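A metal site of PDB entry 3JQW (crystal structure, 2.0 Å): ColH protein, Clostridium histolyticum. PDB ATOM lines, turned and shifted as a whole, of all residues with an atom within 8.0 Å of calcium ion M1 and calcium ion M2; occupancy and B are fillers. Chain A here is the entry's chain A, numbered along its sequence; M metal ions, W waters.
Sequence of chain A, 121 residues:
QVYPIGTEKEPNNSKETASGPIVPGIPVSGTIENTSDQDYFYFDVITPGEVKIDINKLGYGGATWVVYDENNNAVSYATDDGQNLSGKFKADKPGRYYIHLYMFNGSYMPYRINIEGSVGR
Within 4 Å of calcium ion M2: Glu 8, Glu 10, Thr 31, Asp 37 and Asp 39.
Calcium ion M1 is bound by the side-chain carboxylate (OD1) of Asp 37 (2.3 Å), the side-chain carboxylate (OD1) of Asp 39 (2.3 Å), the side-chain amide oxygen (OD1) of Asn 12 (2.4 Å), the side-chain amide oxygen (OD1) of Asn 13 (2.4 Å), the backbone carbonyl oxygen (O) of Gln 38 (2.4 Å), the side-chain carboxylate (OE2) of Glu 10 (2.5 Å) and the side-chain carboxylate (OE1) of Glu 10 (2.6 Å).
Calcium ion M2 is bound by OE2 of Glu 10 (2.3 Å), O of Thr 31 (2.4 Å), water W1 (2.4 Å), OD2 of Asp 39 (2.5 Å), OD2 of Asp 37 (2.5 Å), OE2 of Glu 8 (2.5 Å), OD1 of Asp 39 (2.6 Å) and OE1 of Glu 8 (2.6 Å). Calcium ion M2 has eight donor atoms within binding distance.
OH of Tyr 111 sits close to OE1 of Glu 8 (3.3 Å). The side-chain amide nitrogen (ND2) of Asn 12 sits close to the side-chain carboxylate (OE1) of Glu 8 (3.0 Å). The backbone NH of Glu 8 is in hydrogen-bond range of the backbone carbonyl oxygen of Ser 29. The side-chain hydroxyl of Thr 17 is in hydrogen-bond range of the backbone NH of Asn 13. O of Asp 39 sits at hydrogen-bond distance from N of Leu 101 (2.9 Å). The side-chain carboxylate (OD2) of Asp 37 sits close to the backbone NH (N) of Glu 33 (3.2 Å). The side-chain carboxylate (OD2) of Asp 39 sits close to the side-chain hydroxyl (OH) of Tyr 111, 2.7 Å away. The backbone carbonyl oxygen (O) of Asn 12 lies within hydrogen-bond range of the backbone NH (N) of Tyr 40, 2.9 Å away.
Of the 24 residues printed, 6 come within 4 Å of calcium ion M1.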
ATOM      1  N   GLU A   8      17.523  26.931  -7.814  1.00  0.00           N
ATOM      2  CA  GLU A   8      17.793  25.588  -8.279  1.00  0.00           C
ATOM      3  C   GLU A   8      17.036  24.513  -7.506  1.00  0.00           C
ATOM      4  O   GLU A   8      16.600  24.712  -6.372  1.00  0.00           O
ATOM      5  CB  GLU A   8      19.307  25.280  -8.309  1.00  0.00           C
ATOM      6  CG  GLU A   8      19.997  25.295  -6.939  1.00  0.00           C
ATOM      7  CD  GLU A   8      21.417  24.753  -6.979  1.00  0.00           C
ATOM      8  OE1 GLU A   8      21.766  24.006  -7.947  1.00  0.00           O
ATOM      9  OE2 GLU A   8      22.183  25.022  -6.022  1.00  0.00           O
ATOM     10  N   LYS A   9      16.898  23.343  -8.117  1.00  0.00           N
ATOM     11  CA  LYS A   9      16.289  22.237  -7.455  1.00  0.00           C
ATOM     12  C   LYS A   9      17.147  21.017  -7.624  1.00  0.00           C
ATOM     13  O   LYS A   9      17.155  20.419  -8.685  1.00  0.00           O
ATOM     14  CB  LYS A   9      14.869  21.996  -8.008  1.00  0.00           C
ATOM     15  CG  LYS A   9      14.097  20.938  -7.262  1.00  0.00           C
ATOM     16  CD  LYS A   9      12.640  21.401  -7.051  1.00  0.00           C
ATOM     17  CE  LYS A   9      11.799  20.301  -6.393  1.00  0.00           C
ATOM     18  NZ  LYS A   9      12.602  19.513  -5.386  1.00  0.00           N
ATOM     19  N   GLU A  10      17.875  20.642  -6.562  1.00  0.00           N
ATOM     20  CA  GLU A  10      18.777  19.512  -6.598  1.00  0.00           C
ATOM     21  C   GLU A  10      17.937  18.255  -6.509  1.00  0.00           C
ATOM     22  O   GLU A  10      16.867  18.301  -5.891  1.00  0.00           O
ATOM     23  CB  GLU A  10      19.842  19.572  -5.477  1.00  0.00           C
ATOM     24  CG  GLU A  10      20.864  20.716  -5.617  1.00  0.00           C
ATOM     25  CD  GLU A  10      21.956  20.446  -6.657  1.00  0.00           C
ATOM     26  OE1 GLU A  10      21.947  19.371  -7.282  1.00  0.00           O
ATOM     27  OE2 GLU A  10      22.821  21.333  -6.865  1.00  0.00           O
ATOM     28  N   PRO A  11      18.344  17.155  -7.192  1.00  0.00           N
ATOM     29  CA  PRO A  11      19.545  17.068  -8.077  1.00  0.00           C
ATOM     30  C   PRO A  11      19.307  17.639  -9.472  1.00  0.00           C
ATOM     31  O   PRO A  11      18.291  17.371 -10.095  1.00  0.00           O
ATOM     32  CB  PRO A  11      19.819  15.576  -8.147  1.00  0.00           C
ATOM     33  CG  PRO A  11      18.418  14.917  -7.940  1.00  0.00           C
ATOM     34  CD  PRO A  11      17.605  15.883  -7.097  1.00  0.00           C
ATOM     35  N   ASN A  12      20.236  18.444  -9.959  1.00  0.00           N
ATOM     36  CA  ASN A  12      20.139  19.019 -11.292  1.00  0.00           C
ATOM     37  C   ASN A  12      21.501  18.844 -12.020  1.00  0.00           C
ATOM     38  O   ASN A  12      21.985  19.744 -12.653  1.00  0.00           O
ATOM     39  CB  ASN A  12      19.769  20.509 -11.214  1.00  0.00           C
ATOM     40  CG  ASN A  12      20.803  21.328 -10.421  1.00  0.00           C
ATOM     41  OD1 ASN A  12      21.773  20.758  -9.936  1.00  0.00           O
ATOM     42  ND2 ASN A  12      20.603  22.639 -10.334  1.00  0.00           N
ATOM     43  N   ASN A  13      22.100  17.659 -11.876  1.00  0.00           N
ATOM     44  CA  ASN A  13      23.503  17.437 -12.187  1.00  0.00           C
ATOM     45  C   ASN A  13      23.712  16.908 -13.596  1.00  0.00           C
ATOM     46  O   ASN A  13      24.825  16.557 -13.977  1.00  0.00           O
ATOM     47  CB  ASN A  13      24.147  16.470 -11.189  1.00  0.00           C
ATOM     48  CG  ASN A  13      23.811  16.819  -9.754  1.00  0.00           C
ATOM     49  OD1 ASN A  13      23.984  17.944  -9.315  1.00  0.00           O
ATOM     50  ND2 ASN A  13      23.345  15.816  -8.995  1.00  0.00           N
ATOM     51  N   SER A  14      22.629  16.875 -14.377  1.00  0.00           N
ATOM     52  CA  SER A  14      22.703  16.532 -15.787  1.00  0.00           C
ATOM     53  C   SER A  14      21.686  17.369 -16.555  1.00  0.00           C
ATOM     54  O   SER A  14      20.748  17.965 -15.979  1.00  0.00           O
ATOM     55  CB  SER A  14      22.401  15.039 -15.989  1.00  0.00           C
ATOM     56  OG  SER A  14      21.046  14.799 -15.646  1.00  0.00           O
ATOM     57  N   THR A  17      18.145  16.496 -15.843  1.00  0.00           N
ATOM     58  CA  THR A  17      17.573  16.965 -14.552  1.00  0.00           C
ATOM     59  C   THR A  17      17.707  18.463 -14.326  1.00  0.00           C
ATOM     60  O   THR A  17      17.632  18.930 -13.192  1.00  0.00           O
ATOM     61  CB  THR A  17      18.176  16.232 -13.335  1.00  0.00           C
ATOM     62  OG1 THR A  17      19.613  16.187 -13.439  1.00  0.00           O
ATOM     63  CG2 THR A  17      17.612  14.824 -13.205  1.00  0.00           C
ATOM     64  N   SER A  19      17.296  22.386 -13.841  1.00  0.00           N
ATOM     65  CA  SER A  19      16.273  23.184 -13.127  1.00  0.00           C
ATOM     66  C   SER A  19      15.761  24.252 -14.073  1.00  0.00           C
ATOM     67  O   SER A  19      16.560  24.934 -14.674  1.00  0.00           O
ATOM     68  CB  SER A  19      16.877  23.915 -11.903  1.00  0.00           C
ATOM     69  OG  SER A  19      17.444  23.032 -10.958  1.00  0.00           O
ATOM     70  N   SER A  29      18.576  31.689  -7.551  1.00  0.00           N
ATOM     71  CA  SER A  29      19.631  31.519  -6.557  1.00  0.00           C
ATOM     72  C   SER A  29      20.084  30.082  -6.586  1.00  0.00           C
ATOM     73  O   SER A  29      19.290  29.203  -6.826  1.00  0.00           O
ATOM     74  CB  SER A  29      19.068  31.770  -5.184  1.00  0.00           C
ATOM     75  OG  SER A  29      18.924  33.177  -5.045  1.00  0.00           O
ATOM     76  N   GLY A  30      21.317  29.833  -6.200  1.00  0.00           N
ATOM     77  CA  GLY A  30      21.730  28.454  -5.945  1.00  0.00           C
ATOM     78  C   GLY A  30      23.109  28.489  -5.353  1.00  0.00           C
ATOM     79  O   GLY A  30      23.593  29.569  -5.023  1.00  0.00           O
ATOM     80  N   THR A  31      23.726  27.329  -5.230  1.00  0.00           N
ATOM     81  CA  THR A  31      25.029  27.179  -4.617  1.00  0.00           C
ATOM     82  C   THR A  31      25.759  26.035  -5.310  1.00  0.00           C
ATOM     83  O   THR A  31      25.141  24.966  -5.545  1.00  0.00           O
ATOM     84  CB  THR A  31      24.890  26.858  -3.081  1.00  0.00           C
ATOM     85  OG1 THR A  31      24.305  27.995  -2.417  1.00  0.00           O
ATOM     86  CG2 THR A  31      26.221  26.641  -2.468  1.00  0.00           C
ATOM     87  N   ILE A  32      27.013  26.259  -5.691  1.00  0.00           N
ATOM     88  CA  ILE A  32      27.856  25.153  -6.100  1.00  0.00           C
ATOM     89  C   ILE A  32      28.472  24.604  -4.814  1.00  0.00           C
ATOM     90  O   ILE A  32      29.306  25.257  -4.223  1.00  0.00           O
ATOM     91  CB  ILE A  32      28.914  25.534  -7.143  1.00  0.00           C
ATOM     92  CG1 ILE A  32      28.263  26.306  -8.299  1.00  0.00           C
ATOM     93  CG2 ILE A  32      29.634  24.297  -7.710  1.00  0.00           C
ATOM     94  CD1 ILE A  32      29.323  27.045  -9.191  1.00  0.00           C
ATOM     95  N   GLU A  33      27.977  23.440  -4.363  1.00  0.00           N
ATOM     96  CA  GLU A  33      28.350  22.865  -3.051  1.00  0.00           C
ATOM     97  C   GLU A  33      29.835  22.587  -2.902  1.00  0.00           C
ATOM     98  O   GLU A  33      30.394  22.719  -1.815  1.00  0.00           O
ATOM     99  CB  GLU A  33      27.553  21.604  -2.766  1.00  0.00           C
ATOM    100  CG  GLU A  33      26.076  21.865  -2.653  1.00  0.00           C
ATOM    101  CD  GLU A  33      25.700  22.643  -1.399  1.00  0.00           C
ATOM    102  OE1 GLU A  33      26.382  22.466  -0.334  1.00  0.00           O
ATOM    103  OE2 GLU A  33      24.719  23.439  -1.450  1.00  0.00           O
ATOM    104  N   ASN A  34      30.466  22.192  -4.009  1.00  0.00           N
ATOM    105  CA  ASN A  34      31.883  21.938  -4.085  1.00  0.00           C
ATOM    106  C   ASN A  34      32.129  21.636  -5.556  1.00  0.00           C
ATOM    107  O   ASN A  34      31.178  21.644  -6.328  1.00  0.00           O
ATOM    108  CB  ASN A  34      32.305  20.769  -3.174  1.00  0.00           C
ATOM    109  CG  ASN A  34      31.412  19.522  -3.345  1.00  0.00           C
ATOM    110  OD1 ASN A  34      31.239  19.014  -4.438  1.00  0.00           O
ATOM    111  ND2 ASN A  34      30.890  19.005  -2.246  1.00  0.00           N
ATOM    112  N   SER A  36      32.514  19.020  -7.250  1.00  0.00           N
ATOM    113  CA  SER A  36      31.745  17.894  -7.802  1.00  0.00           C
ATOM    114  C   SER A  36      30.267  18.197  -8.101  1.00  0.00           C
ATOM    115  O   SER A  36      29.593  17.398  -8.758  1.00  0.00           O
ATOM    116  CB  SER A  36      31.825  16.688  -6.859  1.00  0.00           C
ATOM    117  OG  SER A  36      33.164  16.240  -6.725  1.00  0.00           O
ATOM    118  N   ASP A  37      29.765  19.333  -7.620  1.00  0.00           N
ATOM    119  CA  ASP A  37      28.382  19.689  -7.856  1.00  0.00           C
ATOM    120  C   ASP A  37      28.248  20.429  -9.199  1.00  0.00           C
ATOM    121  O   ASP A  37      28.740  21.548  -9.367  1.00  0.00           O
ATOM    122  CB  ASP A  37      27.900  20.595  -6.740  1.00  0.00           C
ATOM    123  CG  ASP A  37      26.421  20.917  -6.861  1.00  0.00           C
ATOM    124  OD1 ASP A  37      25.639  20.111  -7.405  1.00  0.00           O
ATOM    125  OD2 ASP A  37      26.034  21.988  -6.379  1.00  0.00           O
ATOM    126  N   GLN A  38      27.649  19.765 -10.173  1.00  0.00           N
ATOM    127  CA  GLN A  38      27.388  20.386 -11.445  1.00  0.00           C
ATOM    128  C   GLN A  38      25.977  20.922 -11.341  1.00  0.00           C
ATOM    129  O   GLN A  38      25.084  20.218 -10.856  1.00  0.00           O
ATOM    130  CB  GLN A  38      27.464  19.327 -12.579  1.00  0.00           C
ATOM    131  CG  GLN A  38      28.791  18.494 -12.607  1.00  0.00           C
ATOM    132  CD  GLN A  38      29.928  19.289 -13.170  1.00  0.00           C
ATOM    133  OE1 GLN A  38      29.727  20.064 -14.090  1.00  0.00           O
ATOM    134  NE2 GLN A  38      31.113  19.081 -12.646  1.00  0.00           N
ATOM    135  N   ASP A  39      25.744  22.130 -11.841  1.00  0.00           N
ATOM    136  CA  ASP A  39      24.396  22.697 -11.815  1.00  0.00           C
ATOM    137  C   ASP A  39      23.907  23.010 -13.246  1.00  0.00           C
ATOM    138  O   ASP A  39      24.437  23.892 -13.903  1.00  0.00           O
ATOM    139  CB  ASP A  39      24.334  23.952 -10.950  1.00  0.00           C
ATOM    140  CG  ASP A  39      24.482  23.664  -9.443  1.00  0.00           C
ATOM    141  OD1 ASP A  39      24.483  22.492  -9.022  1.00  0.00           O
ATOM    142  OD2 ASP A  39      24.571  24.602  -8.665  1.00  0.00           O
ATOM    143  N   TYR A  40      22.864  22.303 -13.689  1.00  0.00           N
ATOM    144  CA  TYR A  40      22.286  22.570 -14.987  1.00  0.00           C
ATOM    145  C   TYR A  40      20.916  23.221 -14.837  1.00  0.00           C
ATOM    146  O   TYR A  40      20.108  22.831 -13.939  1.00  0.00           O
ATOM    147  CB  TYR A  40      22.120  21.268 -15.809  1.00  0.00           C
ATOM    148  CG  TYR A  40      23.389  20.587 -16.271  1.00  0.00           C
ATOM    149  CD1 TYR A  40      23.780  20.624 -17.613  1.00  0.00           C
ATOM    150  CD2 TYR A  40      24.158  19.855 -15.376  1.00  0.00           C
ATOM    151  CE1 TYR A  40      24.955  19.975 -18.042  1.00  0.00           C
ATOM    152  CE2 TYR A  40      25.289  19.197 -15.770  1.00  0.00           C
ATOM    153  CZ  TYR A  40      25.691  19.237 -17.100  1.00  0.00           C
ATOM    154  OH  TYR A  40      26.833  18.551 -17.439  1.00  0.00           O
ATOM    155  N   PHE A  41      20.674  24.178 -15.749  1.00  0.00           N
ATOM    156  CA  PHE A  41      19.416  24.969 -15.792  1.00  0.00           C
ATOM    157  C   PHE A  41      18.920  24.994 -17.211  1.00  0.00           C
ATOM    158  O   PHE A  41      19.700  24.743 -18.131  1.00  0.00           O
ATOM    159  CB  PHE A  41      19.646  26.403 -15.353  1.00  0.00           C
ATOM    160  CG  PHE A  41      20.106  26.515 -13.932  1.00  0.00           C
ATOM    161  CD1 PHE A  41      19.171  26.658 -12.887  1.00  0.00           C
ATOM    162  CD2 PHE A  41      21.457  26.422 -13.614  1.00  0.00           C
ATOM    163  CE1 PHE A  41      19.593  26.755 -11.562  1.00  0.00           C
ATOM    164  CE2 PHE A  41      21.899  26.518 -12.308  1.00  0.00           C
ATOM    165  CZ  PHE A  41      20.960  26.680 -11.278  1.00  0.00           C
ATOM    166  N   LEU A 101      26.535  25.095 -15.489  1.00  0.00           N
ATOM    167  CA  LEU A 101      27.335  25.876 -14.535  1.00  0.00           C
ATOM    168  C   LEU A 101      28.172  24.949 -13.638  1.00  0.00           C
ATOM    169  O   LEU A 101      27.658  23.996 -13.102  1.00  0.00           O
ATOM    170  CB  LEU A 101      26.423  26.774 -13.663  1.00  0.00           C
ATOM    171  CG  LEU A 101      27.021  27.609 -12.521  1.00  0.00           C
ATOM    172  CD1 LEU A 101      28.010  28.642 -13.004  1.00  0.00           C
ATOM    173  CD2 LEU A 101      25.936  28.314 -11.579  1.00  0.00           C
ATOM    174  N   MET A 109      30.327  27.914  -3.462  1.00  0.00           N
ATOM    175  CA  MET A 109      30.007  29.154  -4.131  1.00  0.00           C
ATOM    176  C   MET A 109      28.533  29.404  -4.331  1.00  0.00           C
ATOM    177  O   MET A 109      27.963  28.880  -5.284  1.00  0.00           O
ATOM    178  CB  MET A 109      30.700  29.237  -5.518  1.00  0.00           C
ATOM    179  CG  MET A 109      30.689  30.712  -6.033  1.00  0.00           C
ATOM    180  SD  MET A 109      31.296  30.713  -7.674  1.00  0.00           S
ATOM    181  CE  MET A 109      33.050  30.619  -7.406  1.00  0.00           C
ATOM    182  N   TYR A 111      25.514  31.643  -5.736  1.00  0.00           N
ATOM    183  CA  TYR A 111      25.484  32.462  -6.974  1.00  0.00           C
ATOM    184  C   TYR A 111      24.063  32.954  -7.230  1.00  0.00           C
ATOM    185  O   TYR A 111      23.100  32.523  -6.568  1.00  0.00           O
ATOM    186  CB  TYR A 111      26.018  31.678  -8.212  1.00  0.00           C
ATOM    187  CG  TYR A 111      25.239  30.397  -8.456  1.00  0.00           C
ATOM    188  CD1 TYR A 111      23.984  30.410  -9.081  1.00  0.00           C
ATOM    189  CD2 TYR A 111      25.709  29.197  -7.991  1.00  0.00           C
ATOM    190  CE1 TYR A 111      23.261  29.224  -9.274  1.00  0.00           C
ATOM    191  CE2 TYR A 111      25.027  28.007  -8.180  1.00  0.00           C
ATOM    192  CZ  TYR A 111      23.807  28.031  -8.807  1.00  0.00           C
ATOM    193  OH  TYR A 111      23.163  26.856  -8.955  1.00  0.00           O
HETATM  194 CA    CA M   1      23.815  20.256  -8.861  1.00  0.00          CA
HETATM  195 CA    CA M   2      23.924  23.286  -6.660  1.00  0.00          CA
HETATM  196  O   HOH W   1      23.578  22.834  -4.307  1.00  0.00           O
